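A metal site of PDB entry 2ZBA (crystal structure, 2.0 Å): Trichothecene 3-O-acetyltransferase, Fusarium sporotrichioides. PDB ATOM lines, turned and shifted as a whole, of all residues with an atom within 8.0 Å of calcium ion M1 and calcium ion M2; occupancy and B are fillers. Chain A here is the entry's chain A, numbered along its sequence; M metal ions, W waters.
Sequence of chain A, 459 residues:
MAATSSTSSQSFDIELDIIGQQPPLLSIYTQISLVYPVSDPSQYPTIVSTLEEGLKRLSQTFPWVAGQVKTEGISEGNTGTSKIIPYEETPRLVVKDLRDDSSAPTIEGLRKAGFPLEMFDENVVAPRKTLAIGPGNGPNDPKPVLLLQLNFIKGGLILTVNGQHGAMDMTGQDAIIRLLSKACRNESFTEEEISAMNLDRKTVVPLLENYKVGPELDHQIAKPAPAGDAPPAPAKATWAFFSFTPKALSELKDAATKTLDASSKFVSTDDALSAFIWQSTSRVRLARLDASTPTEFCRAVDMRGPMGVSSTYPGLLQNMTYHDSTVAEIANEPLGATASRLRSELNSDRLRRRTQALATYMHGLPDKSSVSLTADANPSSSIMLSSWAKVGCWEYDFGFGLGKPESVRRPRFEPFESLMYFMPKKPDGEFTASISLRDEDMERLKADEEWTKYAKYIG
Calcium ion M1 is bound by O of Ile 221 (2.2 Å), O of Asp 218 (2.4 Å), OD1 of Asp 218 (2.5 Å), water W4 (2.5 Å), OD1 of Asp 376 (2.6 Å) and OD2 of Asp 376 (2.7 Å).
Water W3 is bound to calcium ion M2 (2.2 Å). Calcium ion M2 is bound by water W2 (2.2 Å). Calcium ion M2 is bound by OD1 of Asp 218, at 2.5 Å. Water W1 is bound to calcium ion M2 (2.5 Å). OD2 of Asp 218 is bound to calcium ion M2.
Three residues have an atom within 4 Å of calcium ion M1: Asp 218, Ile 221 and Asp 376.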
ATOM      1  N   PRO A 215      -6.325 -11.041 -11.728  1.00  0.00           N
ATOM      2  CA  PRO A 215      -7.217 -10.954 -12.918  1.00  0.00           C
ATOM      3  C   PRO A 215      -8.692 -11.221 -12.692  1.00  0.00           C
ATOM      4  O   PRO A 215      -9.509 -10.770 -13.499  1.00  0.00           O
ATOM      5  CB  PRO A 215      -6.631 -12.006 -13.858  1.00  0.00           C
ATOM      6  CG  PRO A 215      -5.171 -12.017 -13.518  1.00  0.00           C
ATOM      7  CD  PRO A 215      -5.163 -11.920 -12.005  1.00  0.00           C
ATOM      8  N   LEU A 217     -10.677  -9.946 -10.610  1.00  0.00           N
ATOM      9  CA  LEU A 217     -11.410  -8.705 -10.325  1.00  0.00           C
ATOM     10  C   LEU A 217     -11.302  -7.615 -11.393  1.00  0.00           C
ATOM     11  O   LEU A 217     -11.833  -6.512 -11.237  1.00  0.00           O
ATOM     12  CB  LEU A 217     -11.046  -8.169  -8.931  1.00  0.00           C
ATOM     13  CG  LEU A 217     -11.478  -9.031  -7.736  1.00  0.00           C
ATOM     14  CD1 LEU A 217     -11.468  -8.205  -6.509  1.00  0.00           C
ATOM     15  CD2 LEU A 217     -12.864  -9.694  -7.886  1.00  0.00           C
ATOM     16  N   ASP A 218     -10.661  -7.937 -12.505  1.00  0.00           N
ATOM     17  CA  ASP A 218     -10.493  -7.010 -13.630  1.00  0.00           C
ATOM     18  C   ASP A 218     -11.821  -6.346 -14.055  1.00  0.00           C
ATOM     19  O   ASP A 218     -11.919  -5.119 -14.092  1.00  0.00           O
ATOM     20  CB  ASP A 218      -9.825  -7.717 -14.799  1.00  0.00           C
ATOM     21  CG  ASP A 218      -9.805  -6.873 -16.077  1.00  0.00           C
ATOM     22  OD1 ASP A 218      -9.863  -5.618 -16.059  1.00  0.00           O
ATOM     23  OD2 ASP A 218      -9.674  -7.495 -17.134  1.00  0.00           O
ATOM     24  N   HIS A 219     -12.852  -7.147 -14.302  1.00  0.00           N
ATOM     25  CA  HIS A 219     -14.158  -6.604 -14.738  1.00  0.00           C
ATOM     26  C   HIS A 219     -14.829  -5.664 -13.736  1.00  0.00           C
ATOM     27  O   HIS A 219     -15.795  -4.952 -14.089  1.00  0.00           O
ATOM     28  CB  HIS A 219     -15.154  -7.727 -15.005  1.00  0.00           C
ATOM     29  CG  HIS A 219     -14.815  -8.597 -16.179  1.00  0.00           C
ATOM     30  ND1 HIS A 219     -14.884  -8.148 -17.475  1.00  0.00           N
ATOM     31  CD2 HIS A 219     -14.504  -9.909 -16.237  1.00  0.00           C
ATOM     32  CE1 HIS A 219     -14.570  -9.143 -18.294  1.00  0.00           C
ATOM     33  NE2 HIS A 219     -14.336 -10.219 -17.567  1.00  0.00           N
ATOM     34  N   GLN A 220     -14.355  -5.676 -12.504  1.00  0.00           N
ATOM     35  CA  GLN A 220     -14.930  -4.808 -11.470  1.00  0.00           C
ATOM     36  C   GLN A 220     -13.990  -3.708 -10.991  1.00  0.00           C
ATOM     37  O   GLN A 220     -14.280  -3.035 -10.019  1.00  0.00           O
ATOM     38  CB  GLN A 220     -15.508  -5.625 -10.310  1.00  0.00           C
ATOM     39  CG  GLN A 220     -16.411  -6.759 -10.856  1.00  0.00           C
ATOM     40  CD  GLN A 220     -16.858  -7.752  -9.807  1.00  0.00           C
ATOM     41  OE1 GLN A 220     -16.101  -8.128  -8.933  1.00  0.00           O
ATOM     42  NE2 GLN A 220     -18.092  -8.242  -9.957  1.00  0.00           N
ATOM     43  N   ILE A 221     -12.879  -3.493 -11.714  1.00  0.00           N
ATOM     44  CA  ILE A 221     -11.940  -2.393 -11.411  1.00  0.00           C
ATOM     45  C   ILE A 221     -11.581  -1.623 -12.676  1.00  0.00           C
ATOM     46  O   ILE A 221     -11.282  -2.254 -13.699  1.00  0.00           O
ATOM     47  CB  ILE A 221     -10.629  -2.901 -10.719  1.00  0.00           C
ATOM     48  CG1 ILE A 221     -10.955  -3.656  -9.421  1.00  0.00           C
ATOM     49  CG2 ILE A 221      -9.688  -1.693 -10.385  1.00  0.00           C
ATOM     50  CD1 ILE A 221      -9.882  -4.662  -8.989  1.00  0.00           C
ATOM     51  N   ALA A 222     -11.637  -0.292 -12.601  1.00  0.00           N
ATOM     52  CA  ALA A 222     -11.274   0.634 -13.704  1.00  0.00           C
ATOM     53  C   ALA A 222     -11.015   1.995 -13.005  1.00  0.00           C
ATOM     54  O   ALA A 222     -11.519   2.150 -11.910  1.00  0.00           O
ATOM     55  CB  ALA A 222     -12.395   0.694 -14.738  1.00  0.00           C
ATOM     56  N   LYS A 223     -10.337   3.022 -13.534  1.00  0.00           N
ATOM     57  CA  LYS A 223     -10.409   3.662 -14.879  1.00  0.00           C
ATOM     58  C   LYS A 223     -10.979   5.060 -14.604  1.00  0.00           C
ATOM     59  O   LYS A 223     -11.249   5.407 -13.443  1.00  0.00           O
ATOM     60  CB  LYS A 223     -11.321   2.966 -15.884  1.00  0.00           C
ATOM     61  N   GLU A 296     -19.097  -6.667 -24.299  1.00  0.00           N
ATOM     62  CA  GLU A 296     -19.188  -7.300 -22.979  1.00  0.00           C
ATOM     63  C   GLU A 296     -20.653  -7.403 -22.521  1.00  0.00           C
ATOM     64  O   GLU A 296     -21.396  -6.412 -22.552  1.00  0.00           O
ATOM     65  CB  GLU A 296     -18.352  -6.548 -21.951  1.00  0.00           C
ATOM     66  CG  GLU A 296     -18.316  -7.161 -20.519  1.00  0.00           C
ATOM     67  CD  GLU A 296     -17.133  -6.672 -19.690  1.00  0.00           C
ATOM     68  OE1 GLU A 296     -17.340  -5.908 -18.727  1.00  0.00           O
ATOM     69  OE2 GLU A 296     -15.974  -7.046 -19.997  1.00  0.00           O
ATOM     70  N   ASP A 324     -17.112 -11.632 -22.619  1.00  0.00           N
ATOM     71  CA  ASP A 324     -16.502 -10.839 -23.674  1.00  0.00           C
ATOM     72  C   ASP A 324     -16.451 -11.607 -24.978  1.00  0.00           C
ATOM     73  O   ASP A 324     -16.148 -12.802 -24.974  1.00  0.00           O
ATOM     74  CB  ASP A 324     -15.091 -10.411 -23.287  1.00  0.00           C
ATOM     75  CG  ASP A 324     -15.066  -9.560 -22.061  1.00  0.00           C
ATOM     76  OD1 ASP A 324     -15.628  -8.448 -22.086  1.00  0.00           O
ATOM     77  OD2 ASP A 324     -14.466  -9.993 -21.068  1.00  0.00           O
ATOM     78  N   SER A 370     -12.536   2.989  -7.554  1.00  0.00           N
ATOM     79  CA  SER A 370     -12.336   2.281  -8.817  1.00  0.00           C
ATOM     80  C   SER A 370     -13.196   1.018  -8.940  1.00  0.00           C
ATOM     81  O   SER A 370     -13.196   0.360  -9.981  1.00  0.00           O
ATOM     82  CB  SER A 370     -10.845   1.951  -9.024  1.00  0.00           C
ATOM     83  OG  SER A 370     -10.328   1.132  -7.979  1.00  0.00           O
ATOM     84  N   SER A 372     -16.615  -1.049  -9.237  1.00  0.00           N
ATOM     85  CA  SER A 372     -17.980  -1.013  -9.753  1.00  0.00           C
ATOM     86  C   SER A 372     -18.340  -2.335 -10.420  1.00  0.00           C
ATOM     87  O   SER A 372     -17.526  -2.909 -11.135  1.00  0.00           O
ATOM     88  CB  SER A 372     -18.138   0.135 -10.761  1.00  0.00           C
ATOM     89  OG  SER A 372     -19.340   0.028 -11.492  1.00  0.00           O
ATOM     90  N   ALA A 375     -17.641  -1.852 -14.085  1.00  0.00           N
ATOM     91  CA  ALA A 375     -16.402  -1.066 -14.265  1.00  0.00           C
ATOM     92  C   ALA A 375     -15.877  -1.012 -15.712  1.00  0.00           C
ATOM     93  O   ALA A 375     -15.469   0.068 -16.170  1.00  0.00           O
ATOM     94  CB  ALA A 375     -15.307  -1.545 -13.302  1.00  0.00           C
ATOM     95  N   ASP A 376     -15.939  -2.137 -16.418  1.00  0.00           N
ATOM     96  CA  ASP A 376     -15.415  -2.244 -17.781  1.00  0.00           C
ATOM     97  C   ASP A 376     -16.481  -2.213 -18.890  1.00  0.00           C
ATOM     98  O   ASP A 376     -16.168  -2.445 -20.054  1.00  0.00           O
ATOM     99  CB  ASP A 376     -14.580  -3.515 -17.943  1.00  0.00           C
ATOM    100  CG  ASP A 376     -13.316  -3.506 -17.098  1.00  0.00           C
ATOM    101  OD1 ASP A 376     -13.037  -2.481 -16.413  1.00  0.00           O
ATOM    102  OD2 ASP A 376     -12.622  -4.535 -17.099  1.00  0.00           O
ATOM    103  N   ALA A 377     -17.728  -1.923 -18.535  1.00  0.00           N
ATOM    104  CA  ALA A 377     -18.817  -1.840 -19.533  1.00  0.00           C
ATOM    105  C   ALA A 377     -18.672  -0.579 -20.406  1.00  0.00           C
ATOM    106  O   ALA A 377     -18.332   0.491 -19.907  1.00  0.00           O
ATOM    107  CB  ALA A 377     -20.164  -1.845 -18.830  1.00  0.00           C
HETATM  108 CA    CA M   1     -10.859  -3.438 -15.449  1.00  0.00          CA
HETATM  109 CA    CA M   2      -9.931  -5.370 -18.549  1.00  0.00          CA
HETATM  110  O   HOH W   1     -11.146  -3.977 -20.254  1.00  0.00           O
HETATM  111  O   HOH W   2      -9.693  -6.811 -20.257  1.00  0.00           O
HETATM  112  O   HOH W   3     -11.930  -6.354 -18.509  1.00  0.00           O
HETATM  113  O   HOH W   4      -8.571  -3.468 -14.502  1.00  0.00           O
